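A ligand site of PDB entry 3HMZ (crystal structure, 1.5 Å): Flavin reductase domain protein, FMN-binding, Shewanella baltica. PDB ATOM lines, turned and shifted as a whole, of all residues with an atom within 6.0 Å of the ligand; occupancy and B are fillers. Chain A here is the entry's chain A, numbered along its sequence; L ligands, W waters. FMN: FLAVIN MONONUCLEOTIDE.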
ATOM      1  N   THR A  31      17.740 -26.044 -22.721  1.00  0.00           N
ATOM      2  CA  THR A  31      16.656 -26.495 -23.564  1.00  0.00           C
ATOM      3  C   THR A  31      15.378 -26.008 -22.876  1.00  0.00           C
ATOM      4  O   THR A  31      15.287 -26.018 -21.642  1.00  0.00           O
ATOM      5  CB  THR A  31      16.720 -28.010 -23.723  1.00  0.00           C
ATOM      6  OG1 THR A  31      17.904 -28.315 -24.476  1.00  0.00           O
ATOM      7  CG2 THR A  31      15.509 -28.528 -24.409  1.00  0.00           C
ATOM      8  N   ASN A  43      -0.818 -25.844 -26.590  1.00  0.00           N
ATOM      9  CA  ASN A  43       0.171 -26.804 -26.949  1.00  0.00           C
ATOM     10  C   ASN A  43       1.516 -26.462 -26.318  1.00  0.00           C
ATOM     11  O   ASN A  43       1.744 -25.325 -25.931  1.00  0.00           O
ATOM     12  CB  ASN A  43       0.360 -26.934 -28.459  1.00  0.00           C
ATOM     13  CG  ASN A  43       0.963 -28.253 -28.872  1.00  0.00           C
ATOM     14  OD1 ASN A  43       0.941 -29.227 -28.121  1.00  0.00           O
ATOM     15  ND2 ASN A  43       1.512 -28.285 -30.087  1.00  0.00           N
ATOM     16  N   VAL A  44       2.329 -27.489 -26.192  1.00  0.00           N
ATOM     17  CA  VAL A  44       3.682 -27.381 -25.652  1.00  0.00           C
ATOM     18  C   VAL A  44       4.580 -28.314 -26.510  1.00  0.00           C
ATOM     19  O   VAL A  44       4.218 -29.441 -26.792  1.00  0.00           O
ATOM     20  CB  VAL A  44       3.756 -27.818 -24.162  1.00  0.00           C
ATOM     21  CG1 VAL A  44       5.227 -27.692 -23.607  1.00  0.00           C
ATOM     22  CG2 VAL A  44       2.701 -27.098 -23.280  1.00  0.00           C
ATOM     23  N   MET A  45       5.769 -27.825 -26.860  1.00  0.00           N
ATOM     24  CA  MET A  45       6.823 -28.634 -27.475  1.00  0.00           C
ATOM     25  C   MET A  45       8.166 -28.300 -26.815  1.00  0.00           C
ATOM     26  O   MET A  45       8.270 -27.338 -26.070  1.00  0.00           O
ATOM     27  CB  MET A  45       6.931 -28.384 -28.987  1.00  0.00           C
ATOM     28  CG  MET A  45       7.290 -26.951 -29.372  1.00  0.00           C
ATOM     29  SD  MET A  45       7.654 -26.731 -31.243  1.00  0.00           S
ATOM     30  CE  MET A  45       9.568 -26.520 -31.218  1.00  0.00           C
ATOM     31  N   ALA A  46       9.165 -29.128 -27.108  1.00  0.00           N
ATOM     32  CA  ALA A  46      10.537 -28.904 -26.640  1.00  0.00           C
ATOM     33  C   ALA A  46      11.313 -28.146 -27.724  1.00  0.00           C
ATOM     34  O   ALA A  46      11.129 -28.385 -28.932  1.00  0.00           O
ATOM     35  CB  ALA A  46      11.242 -30.194 -26.301  1.00  0.00           C
ATOM     36  N   ALA A  47      12.152 -27.202 -27.292  1.00  0.00           N
ATOM     37  CA  ALA A  47      13.070 -26.503 -28.192  1.00  0.00           C
ATOM     38  C   ALA A  47      14.451 -26.340 -27.563  1.00  0.00           C
ATOM     39  O   ALA A  47      14.584 -25.675 -26.529  1.00  0.00           O
ATOM     40  CB  ALA A  47      12.541 -25.123 -28.638  1.00  0.00           C
ATOM     41  N   ALA A  48      15.461 -26.982 -28.159  1.00  0.00           N
ATOM     42  CA  ALA A  48      16.838 -26.689 -27.787  1.00  0.00           C
ATOM     43  C   ALA A  48      17.326 -25.381 -28.411  1.00  0.00           C
ATOM     44  O   ALA A  48      18.202 -24.714 -27.851  1.00  0.00           O
ATOM     45  CB  ALA A  48      17.762 -27.815 -28.216  1.00  0.00           C
ATOM     46  N   TRP A  49      16.765 -25.005 -29.576  1.00  0.00           N
ATOM     47  CA  TRP A  49      17.299 -23.873 -30.355  1.00  0.00           C
ATOM     48  C   TRP A  49      16.603 -22.570 -30.068  1.00  0.00           C
ATOM     49  O   TRP A  49      16.024 -21.942 -30.930  1.00  0.00           O
ATOM     50  CB  TRP A  49      17.338 -24.226 -31.833  1.00  0.00           C
ATOM     51  CG  TRP A  49      18.178 -25.408 -32.159  1.00  0.00           C
ATOM     52  CD1 TRP A  49      19.035 -26.086 -31.327  1.00  0.00           C
ATOM     53  CD2 TRP A  49      18.318 -26.036 -33.429  1.00  0.00           C
ATOM     54  NE1 TRP A  49      19.651 -27.145 -31.983  1.00  0.00           N
ATOM     55  CE2 TRP A  49      19.233 -27.115 -33.286  1.00  0.00           C
ATOM     56  CE3 TRP A  49      17.742 -25.791 -34.691  1.00  0.00           C
ATOM     57  CZ2 TRP A  49      19.559 -27.944 -34.344  1.00  0.00           C
ATOM     58  CZ3 TRP A  49      18.074 -26.632 -35.730  1.00  0.00           C
ATOM     59  CH2 TRP A  49      18.976 -27.684 -35.551  1.00  0.00           C
ATOM     60  N   CYS A  50      16.683 -22.165 -28.806  1.00  0.00           N
ATOM     61  CA  CYS A  50      16.117 -20.928 -28.286  1.00  0.00           C
ATOM     62  C   CYS A  50      17.270 -20.169 -27.647  1.00  0.00           C
ATOM     63  O   CYS A  50      18.004 -20.735 -26.879  1.00  0.00           O
ATOM     64  CB  CYS A  50      15.038 -21.223 -27.254  1.00  0.00           C
ATOM     65  SG  CYS A  50      14.330 -19.691 -26.566  1.00  0.00           S
ATOM     66  N   VAL A  62      13.886 -18.245 -31.528  1.00  0.00           N
ATOM     67  CA  VAL A  62      13.603 -19.684 -31.438  1.00  0.00           C
ATOM     68  C   VAL A  62      13.417 -20.229 -32.860  1.00  0.00           C
ATOM     69  O   VAL A  62      12.876 -19.535 -33.733  1.00  0.00           O
ATOM     70  CB  VAL A  62      12.428 -20.001 -30.503  1.00  0.00           C
ATOM     71  CG1 VAL A  62      11.062 -19.398 -30.995  1.00  0.00           C
ATOM     72  CG2 VAL A  62      12.375 -21.499 -30.253  1.00  0.00           C
ATOM     73  N   VAL A  63      13.932 -21.412 -33.091  1.00  0.00           N
ATOM     74  CA  VAL A  63      13.820 -22.095 -34.366  1.00  0.00           C
ATOM     75  C   VAL A  63      12.667 -23.080 -34.245  1.00  0.00           C
ATOM     76  O   VAL A  63      12.663 -23.939 -33.358  1.00  0.00           O
ATOM     77  CB  VAL A  63      15.119 -22.810 -34.749  1.00  0.00           C
ATOM     78  CG1 VAL A  63      14.975 -23.389 -36.135  1.00  0.00           C
ATOM     79  CG2 VAL A  63      16.300 -21.819 -34.679  1.00  0.00           C
ATOM     80  N   LEU A  64      11.675 -22.947 -35.126  1.00  0.00           N
ATOM     81  CA  LEU A  64      10.469 -23.776 -35.094  1.00  0.00           C
ATOM     82  C   LEU A  64      10.278 -24.451 -36.436  1.00  0.00           C
ATOM     83  O   LEU A  64      10.018 -23.790 -37.438  1.00  0.00           O
ATOM     84  CB  LEU A  64       9.249 -22.941 -34.746  1.00  0.00           C
ATOM     85  CG  LEU A  64       9.312 -22.112 -33.458  1.00  0.00           C
ATOM     86  CD1 LEU A  64       8.117 -21.124 -33.389  1.00  0.00           C
ATOM     87  CD2 LEU A  64       9.389 -23.001 -32.240  1.00  0.00           C
ATOM     88  N   ASP A  65      10.367 -25.763 -36.457  1.00  0.00           N
ATOM     89  CA  ASP A  65      10.230 -26.513 -37.711  1.00  0.00           C
ATOM     90  C   ASP A  65       8.806 -26.337 -38.276  1.00  0.00           C
ATOM     91  O   ASP A  65       7.828 -26.254 -37.542  1.00  0.00           O
ATOM     92  CB  ASP A  65      10.545 -27.966 -37.479  1.00  0.00           C
ATOM     93  CG  ASP A  65      10.705 -28.728 -38.761  1.00  0.00           C
ATOM     94  OD1 ASP A  65       9.674 -29.226 -39.271  1.00  0.00           O
ATOM     95  OD2 ASP A  65      11.858 -28.822 -39.255  1.00  0.00           O
ATOM     96  N   MET A  67       6.906 -28.439 -39.557  1.00  0.00           N
ATOM     97  CA  MET A  67       6.060 -29.604 -39.227  1.00  0.00           C
ATOM     98  C   MET A  67       5.349 -29.425 -37.875  1.00  0.00           C
ATOM     99  O   MET A  67       4.443 -30.199 -37.553  1.00  0.00           O
ATOM    100  CB  MET A  67       6.871 -30.927 -39.178  1.00  0.00           C
ATOM    101  CG  MET A  67       7.679 -31.245 -37.842  1.00  0.00           C
ATOM    102  SD  MET A  67       8.703 -32.935 -37.641  1.00  0.00           S
ATOM    103  CE  MET A  67      10.099 -32.758 -38.998  1.00  0.00           C
ATOM    104  N   THR A  68       5.774 -28.459 -37.069  1.00  0.00           N
ATOM    105  CA  THR A  68       5.214 -28.380 -35.719  1.00  0.00           C
ATOM    106  C   THR A  68       3.886 -27.662 -35.597  1.00  0.00           C
ATOM    107  O   THR A  68       3.660 -26.616 -36.216  1.00  0.00           O
ATOM    108  CB  THR A  68       6.202 -27.756 -34.704  1.00  0.00           C
ATOM    109  OG1 THR A  68       6.383 -26.358 -34.938  1.00  0.00           O
ATOM    110  CG2 THR A  68       7.512 -28.473 -34.661  1.00  0.00           C
ATOM    111  N   LYS A  69       2.989 -28.241 -34.788  1.00  0.00           N
ATOM    112  CA  LYS A  69       1.702 -27.622 -34.512  1.00  0.00           C
ATOM    113  C   LYS A  69       1.918 -26.337 -33.725  1.00  0.00           C
ATOM    114  O   LYS A  69       1.269 -25.345 -33.960  1.00  0.00           O
ATOM    115  CB  LYS A  69       0.753 -28.575 -33.784  1.00  0.00           C
ATOM    116  CG  LYS A  69      -0.656 -28.008 -33.532  1.00  0.00           C
ATOM    117  CD  LYS A  69      -1.420 -27.627 -34.807  1.00  0.00           C
ATOM    118  CE  LYS A  69      -1.761 -28.789 -35.645  1.00  0.00           C
ATOM    119  NZ  LYS A  69      -2.761 -28.299 -36.725  1.00  0.00           N
ATOM    120  N   THR A  70       2.905 -26.335 -32.830  1.00  0.00           N
ATOM    121  CA  THR A  70       3.192 -25.119 -32.054  1.00  0.00           C
ATOM    122  C   THR A  70       3.532 -23.920 -32.948  1.00  0.00           C
ATOM    123  O   THR A  70       3.071 -22.818 -32.692  1.00  0.00           O
ATOM    124  CB  THR A  70       4.289 -25.375 -30.988  1.00  0.00           C
ATOM    125  OG1 THR A  70       3.918 -26.498 -30.202  1.00  0.00           O
ATOM    126  CG2 THR A  70       4.413 -24.172 -30.085  1.00  0.00           C
ATOM    127  N   ARG A  71       4.309 -24.157 -34.009  1.00  0.00           N
ATOM    128  CA  ARG A  71       4.608 -23.067 -34.955  1.00  0.00           C
ATOM    129  C   ARG A  71       3.323 -22.461 -35.543  1.00  0.00           C
ATOM    130  O   ARG A  71       3.176 -21.235 -35.642  1.00  0.00           O
ATOM    131  CB  ARG A  71       5.498 -23.572 -36.066  1.00  0.00           C
ATOM    132  CG  ARG A  71       5.704 -22.560 -37.154  1.00  0.00           C
ATOM    133  CD  ARG A  71       6.711 -23.039 -38.113  1.00  0.00           C
ATOM    134  NE  ARG A  71       6.758 -22.147 -39.287  1.00  0.00           N
ATOM    135  CZ  ARG A  71       7.827 -21.923 -40.038  1.00  0.00           C
ATOM    136  NH1 ARG A  71       9.016 -22.463 -39.732  1.00  0.00           N
ATOM    137  NH2 ARG A  71       7.740 -21.101 -41.108  1.00  0.00           N
ATOM    138  N   THR A  93       9.823 -33.366 -20.881  1.00  0.00           N
ATOM    139  CA  THR A  93      10.536 -32.594 -21.926  1.00  0.00           C
ATOM    140  C   THR A  93      10.763 -33.439 -23.172  1.00  0.00           C
ATOM    141  O   THR A  93      10.456 -33.010 -24.290  1.00  0.00           O
ATOM    142  CB  THR A  93      11.829 -32.017 -21.383  1.00  0.00           C
ATOM    143  OG1 THR A  93      11.530 -31.163 -20.266  1.00  0.00           O
ATOM    144  CG2 THR A  93      12.601 -31.233 -22.450  1.00  0.00           C
ATOM    145  N   HIS A  94      11.232 -34.650 -22.957  1.00  0.00           N
ATOM    146  CA  HIS A  94      11.455 -35.533 -24.079  1.00  0.00           C
ATOM    147  C   HIS A  94      10.149 -35.912 -24.778  1.00  0.00           C
ATOM    148  O   HIS A  94      10.092 -35.926 -26.010  1.00  0.00           O
ATOM    149  CB  HIS A  94      12.221 -36.764 -23.626  1.00  0.00           C
ATOM    150  CG  HIS A  94      12.747 -37.573 -24.764  1.00  0.00           C
ATOM    151  ND1 HIS A  94      12.104 -38.713 -25.147  1.00  0.00           N
ATOM    152  CD2 HIS A  94      13.712 -37.342 -25.678  1.00  0.00           C
ATOM    153  CE1 HIS A  94      12.725 -39.226 -26.200  1.00  0.00           C
ATOM    154  NE2 HIS A  94      13.723 -38.414 -26.545  1.00  0.00           N
ATOM    155  N   ARG A  95       9.098 -36.135 -23.995  1.00  0.00           N
ATOM    156  CA  ARG A  95       7.799 -36.543 -24.545  1.00  0.00           C
ATOM    157  C   ARG A  95       7.166 -35.457 -25.387  1.00  0.00           C
ATOM    158  O   ARG A  95       6.674 -35.741 -26.489  1.00  0.00           O
ATOM    159  CB  ARG A  95       6.829 -36.970 -23.435  1.00  0.00           C
ATOM    160  CG  ARG A  95       7.163 -38.300 -22.806  1.00  0.00           C
ATOM    161  CD  ARG A  95       6.119 -38.636 -21.741  1.00  0.00           C
ATOM    162  NE  ARG A  95       6.506 -39.822 -20.988  1.00  0.00           N
ATOM    163  CZ  ARG A  95       5.706 -40.475 -20.159  1.00  0.00           C
ATOM    164  NH1 ARG A  95       4.459 -40.094 -20.003  1.00  0.00           N
ATOM    165  NH2 ARG A  95       6.161 -41.544 -19.525  1.00  0.00           N
ATOM    166  N   VAL A  96       7.153 -34.219 -24.891  1.00  0.00           N
ATOM    167  CA  VAL A  96       6.549 -33.119 -25.685  1.00  0.00           C
ATOM    168  C   VAL A  96       7.359 -32.805 -26.943  1.00  0.00           C
ATOM    169  O   VAL A  96       6.811 -32.210 -27.863  1.00  0.00           O
ATOM    170  CB  VAL A  96       6.285 -31.821 -24.895  1.00  0.00           C
ATOM    171  CG1 VAL A  96       5.295 -32.108 -23.708  1.00  0.00           C
ATOM    172  CG2 VAL A  96       7.569 -31.183 -24.390  1.00  0.00           C
ATOM    173  N   GLY A  97       8.616 -33.229 -26.954  1.00  0.00           N
ATOM    174  CA  GLY A  97       9.460 -33.111 -28.114  1.00  0.00           C
ATOM    175  C   GLY A  97       9.495 -34.339 -29.020  1.00  0.00           C
ATOM    176  O   GLY A  97      10.252 -34.357 -29.996  1.00  0.00           O
ATOM    177  N   SER A  98       8.681 -35.351 -28.700  1.00  0.00           N
ATOM    178  CA  SER A  98       8.637 -36.607 -29.444  1.00  0.00           C
ATOM    179  C   SER A  98       7.236 -36.973 -29.941  1.00  0.00           C
ATOM    180  O   SER A  98       7.056 -38.032 -30.563  1.00  0.00           O
ATOM    181  CB  SER A  98       9.183 -37.726 -28.567  1.00  0.00           C
ATOM    182  OG  SER A  98      10.493 -37.479 -28.129  1.00  0.00           O
ATOM    183  N   GLN A  99       6.251 -36.106 -29.678  1.00  0.00           N
ATOM    184  CA  GLN A  99       4.841 -36.300 -30.017  1.00  0.00           C
ATOM    185  C   GLN A  99       4.282 -34.996 -30.527  1.00  0.00           C
ATOM    186  O   GLN A  99       4.590 -33.967 -29.933  1.00  0.00           O
ATOM    187  CB  GLN A  99       4.097 -36.684 -28.720  1.00  0.00           C
ATOM    188  CG  GLN A  99       4.573 -37.996 -28.096  1.00  0.00           C
ATOM    189  CD  GLN A  99       3.919 -38.320 -26.765  1.00  0.00           C
ATOM    190  OE1 GLN A  99       2.786 -37.971 -26.514  1.00  0.00           O
ATOM    191  NE2 GLN A  99       4.668 -39.009 -25.903  1.00  0.00           N
ATOM    192  N   SER A 100       3.447 -35.011 -31.567  1.00  0.00           N
ATOM    193  CA  SER A 100       2.808 -33.794 -32.054  1.00  0.00           C
ATOM    194  C   SER A 100       1.341 -33.779 -31.702  1.00  0.00           C
ATOM    195  O   SER A 100       0.657 -34.826 -31.773  1.00  0.00           O
ATOM    196  CB  SER A 100       2.921 -33.663 -33.587  1.00  0.00           C
ATOM    197  OG  SER A 100       2.253 -32.465 -34.070  1.00  0.00           O
ATOM    198  N   LEU A 101       0.868 -32.596 -31.333  1.00  0.00           N
ATOM    199  CA  LEU A 101      -0.549 -32.378 -31.068  1.00  0.00           C
ATOM    200  C   LEU A 101      -1.387 -32.704 -32.304  1.00  0.00           C
ATOM    201  O   LEU A 101      -2.532 -33.105 -32.166  1.00  0.00           O
ATOM    202  CB  LEU A 101      -0.806 -30.934 -30.654  1.00  0.00           C
ATOM    203  CG  LEU A 101      -2.245 -30.574 -30.231  1.00  0.00           C
ATOM    204  CD1 LEU A 101      -2.675 -31.329 -28.981  1.00  0.00           C
ATOM    205  CD2 LEU A 101      -2.317 -29.093 -30.029  1.00  0.00           C
ATOM    206  N   ALA A 102      -0.819 -32.553 -33.511  1.00  0.00           N
ATOM    207  CA  ALA A 102      -1.547 -32.918 -34.747  1.00  0.00           C
ATOM    208  C   ALA A 102      -1.972 -34.406 -34.755  1.00  0.00           C
ATOM    209  O   ALA A 102      -2.986 -34.766 -35.403  1.00  0.00           O
ATOM    210  CB  ALA A 102      -0.697 -32.607 -35.971  1.00  0.00           C
ATOM    211  N   LYS A 107      -2.424 -34.791 -26.362  1.00  0.00           N
ATOM    212  CA  LYS A 107      -0.971 -34.718 -26.134  1.00  0.00           C
ATOM    213  C   LYS A 107      -0.595 -34.307 -24.709  1.00  0.00           C
ATOM    214  O   LYS A 107       0.225 -34.969 -24.073  1.00  0.00           O
ATOM    215  CB  LYS A 107      -0.320 -33.759 -27.135  1.00  0.00           C
ATOM    216  CG  LYS A 107       1.151 -33.554 -26.902  1.00  0.00           C
ATOM    217  CD  LYS A 107       1.785 -32.647 -27.907  1.00  0.00           C
ATOM    218  CE  LYS A 107       3.292 -32.490 -27.580  1.00  0.00           C
ATOM    219  NZ  LYS A 107       3.955 -31.511 -28.512  1.00  0.00           N
ATOM    220  N   TYR A 183      19.954 -30.405 -23.895  1.00  0.00           N
ATOM    221  CA  TYR A 183      19.831 -31.561 -24.776  1.00  0.00           C
ATOM    222  C   TYR A 183      20.999 -31.783 -25.696  1.00  0.00           C
ATOM    223  O   TYR A 183      21.566 -30.829 -26.187  1.00  0.00           O
ATOM    224  CB  TYR A 183      18.597 -31.377 -25.645  1.00  0.00           C
ATOM    225  CG  TYR A 183      18.201 -32.541 -26.499  1.00  0.00           C
ATOM    226  CD1 TYR A 183      17.963 -33.771 -25.936  1.00  0.00           C
ATOM    227  CD2 TYR A 183      17.912 -32.359 -27.856  1.00  0.00           C
ATOM    228  CE1 TYR A 183      17.523 -34.856 -26.712  1.00  0.00           C
ATOM    229  CE2 TYR A 183      17.451 -33.440 -28.632  1.00  0.00           C
ATOM    230  CZ  TYR A 183      17.245 -34.664 -28.045  1.00  0.00           C
ATOM    231  OH  TYR A 183      16.752 -35.704 -28.824  1.00  0.00           O
ATOM    232  N   GLY A 186      18.900 -37.980 -29.070  1.00  0.00           N
ATOM    233  CA  GLY A 186      18.180 -39.138 -28.593  1.00  0.00           C
ATOM    234  C   GLY A 186      17.409 -38.776 -27.354  1.00  0.00           C
ATOM    235  O   GLY A 186      16.651 -37.813 -27.347  1.00  0.00           O
ATOM    236  N   PHE A 189      20.429 -35.854 -22.290  1.00  0.00           N
ATOM    237  CA  PHE A 189      20.596 -34.480 -21.847  1.00  0.00           C
ATOM    238  C   PHE A 189      21.681 -34.415 -20.782  1.00  0.00           C
ATOM    239  O   PHE A 189      22.029 -35.407 -20.148  1.00  0.00           O
ATOM    240  CB  PHE A 189      19.328 -33.986 -21.125  1.00  0.00           C
ATOM    241  CG  PHE A 189      18.054 -33.985 -21.951  1.00  0.00           C
ATOM    242  CD1 PHE A 189      17.360 -35.178 -22.207  1.00  0.00           C
ATOM    243  CD2 PHE A 189      17.473 -32.788 -22.366  1.00  0.00           C
ATOM    244  CE1 PHE A 189      16.177 -35.191 -22.936  1.00  0.00           C
ATOM    245  CE2 PHE A 189      16.252 -32.786 -23.084  1.00  0.00           C
ATOM    246  CZ  PHE A 189      15.601 -33.986 -23.347  1.00  0.00           C
HETATM  247  N1  FMN L   1      11.815 -28.683 -32.785  1.00  0.00           N
HETATM  248  C2  FMN L   1      12.035 -27.421 -33.279  1.00  0.00           C
HETATM  249  O2  FMN L   1      11.346 -27.016 -34.208  1.00  0.00           O
HETATM  250  N3  FMN L   1      13.020 -26.639 -32.690  1.00  0.00           N
HETATM  251  C4  FMN L   1      13.793 -27.067 -31.665  1.00  0.00           C
HETATM  252  O4  FMN L   1      14.679 -26.292 -31.211  1.00  0.00           O
HETATM  253  C4A FMN L   1      13.569 -28.363 -31.181  1.00  0.00           C
HETATM  254  N5  FMN L   1      14.304 -28.875 -30.129  1.00  0.00           N
HETATM  255  C5A FMN L   1      13.977 -30.064 -29.502  1.00  0.00           C
HETATM  256  C6  FMN L   1      14.618 -30.470 -28.328  1.00  0.00           C
HETATM  257  C7  FMN L   1      14.309 -31.682 -27.715  1.00  0.00           C
HETATM  258  C7M FMN L   1      14.989 -32.086 -26.444  1.00  0.00           C
HETATM  259  C8  FMN L   1      13.338 -32.498 -28.281  1.00  0.00           C
HETATM  260  C8M FMN L   1      12.959 -33.832 -27.654  1.00  0.00           C
HETATM  261  C9  FMN L   1      12.695 -32.081 -29.442  1.00  0.00           C
HETATM  262  C9A FMN L   1      12.987 -30.885 -30.081  1.00  0.00           C
HETATM  263  N10 FMN L   1      12.341 -30.441 -31.235  1.00  0.00           N
HETATM  264  C10 FMN L   1      12.577 -29.173 -31.747  1.00  0.00           C
HETATM  265  C1' FMN L   1      11.192 -31.199 -31.843  1.00  0.00           C
HETATM  266  C2' FMN L   1       9.793 -30.744 -31.401  1.00  0.00           C
HETATM  267  O2' FMN L   1       9.727 -30.510 -29.988  1.00  0.00           O
HETATM  268  C3' FMN L   1       8.839 -31.848 -31.833  1.00  0.00           C
HETATM  269  O3' FMN L   1       8.813 -31.905 -33.260  1.00  0.00           O
HETATM  270  C4' FMN L   1       7.435 -31.748 -31.204  1.00  0.00           C
HETATM  271  O4' FMN L   1       6.839 -33.033 -31.309  1.00  0.00           O
HETATM  272  C5' FMN L   1       6.534 -30.706 -31.842  1.00  0.00           C
HETATM  273  O5' FMN L   1       5.265 -30.793 -31.197  1.00  0.00           O
HETATM  274  P   FMN L   1       3.977 -30.084 -31.841  1.00  0.00           P
HETATM  275  O1P FMN L   1       2.847 -30.593 -30.973  1.00  0.00           O
HETATM  276  O2P FMN L   1       4.152 -28.589 -31.823  1.00  0.00           O
HETATM  277  O3P FMN L   1       3.858 -30.561 -33.271  1.00  0.00           O
HETATM  278  O   HOH W   1      10.375 -30.121 -34.994  1.00  0.00           O
HETATM  279  O   HOH W   2       5.382 -31.921 -35.170  1.00  0.00           O
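The side-chain hydroxyl (OG) of Ser 100 lies within hydrogen-bond range of an oxygen (O3P) of the ligand (2.6 Å). O2P of the ligand is in hydrogen-bond range of N of Thr 70 (2.8 Å). An oxygen (O2P) of the ligand lies within hydrogen-bond range of the side-chain hydroxyl (OG1) of Thr 70, at 2.7 Å. The backbone NH (N) of Asp 65 lies within hydrogen-bond range of an oxygen (O2) of the ligand (2.8 Å). N of Ala 46 sits at hydrogen-bond distance from O2' of the ligand, 3.2 Å away. O of Ala 46 is in hydrogen-bond range of O2' of the ligand, 2.8 Å away. The backbone carbonyl oxygen (O) of Gln 99 is in hydrogen-bond range of an oxygen (O4') of the ligand. N3 of the ligand lies within hydrogen-bond range of O of Val 63 (2.8 Å). An oxygen (O1P) of the ligand lies within hydrogen-bond range of the side-chain amide nitrogen (ND2) of Asn 43. N of Leu 101 sits at hydrogen-bond distance from O1P of the ligand, at 2.8 Å. NZ of Lys 107 is in salt-bridge range of O1P of the ligand, at 2.9 Å. An oxygen (O3P) of the ligand lies within hydrogen-bond range of the backbone NH of Lys 69 (2.9 Å). N of Trp 49 is in hydrogen-bond range of O4 of the ligand. The backbone NH (N) of Ala 48 lies within hydrogen-bond range of a nitrogen (N5) of the ligand (3.0 Å).
The backbone carbonyl oxygen (O) of Asp 65 lies within hydrogen-bond range of the side-chain hydroxyl (OG1) of Thr 68 (3.0 Å). OD1 of Asp 65 sits at hydrogen-bond distance from N of Met 67, at 2.9 Å. The side-chain amino group of Lys 107 sits at hydrogen-bond distance from the backbone carbonyl oxygen of Gln 99, at 2.9 Å. O of Trp 49 sits at hydrogen-bond distance from N of Val 63, at 3.1 Å. The side-chain amino group (NZ) of Lys 107 sits at hydrogen-bond distance from the backbone carbonyl oxygen (O) of Val 96 (3.0 Å). NZ of Lys 107 lies within hydrogen-bond range of O of Val 44, 2.7 Å away. The side-chain hydroxyl (OG1) of Thr 68 sits close to the backbone NH (N) of Arg 71 (3.2 Å). O of Gly 186 is in hydrogen-bond range of NE2 of His 94.
Merely in contact with the ligand: Gly 97 (3.2 Å), Tyr 183 (3.2 Å), Ala 47 (3.3 Å), Met 45 (3.3 Å), Val 96 (3.4 Å), Leu 64 (3.5 Å), Thr 68 (3.5 Å), Phe 189 (3.7 Å), His 94 (3.9 Å) and Ser 98 (3.9 Å). Of the 32 residues printed, 22 come within 4 Å of the ligand. Along chain A the residues within 4 Å of the ligand span positions 43 to 189. The nearest printed residue that does not touch the ligand is Thr 31 (4.1 Å).
Water W2 lies within hydrogen-bond range of an oxygen (O3P) of the ligand, the backbone carbonyl oxygen (O) of Met 67 and the side-chain hydroxyl (OG) of Ser 100.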
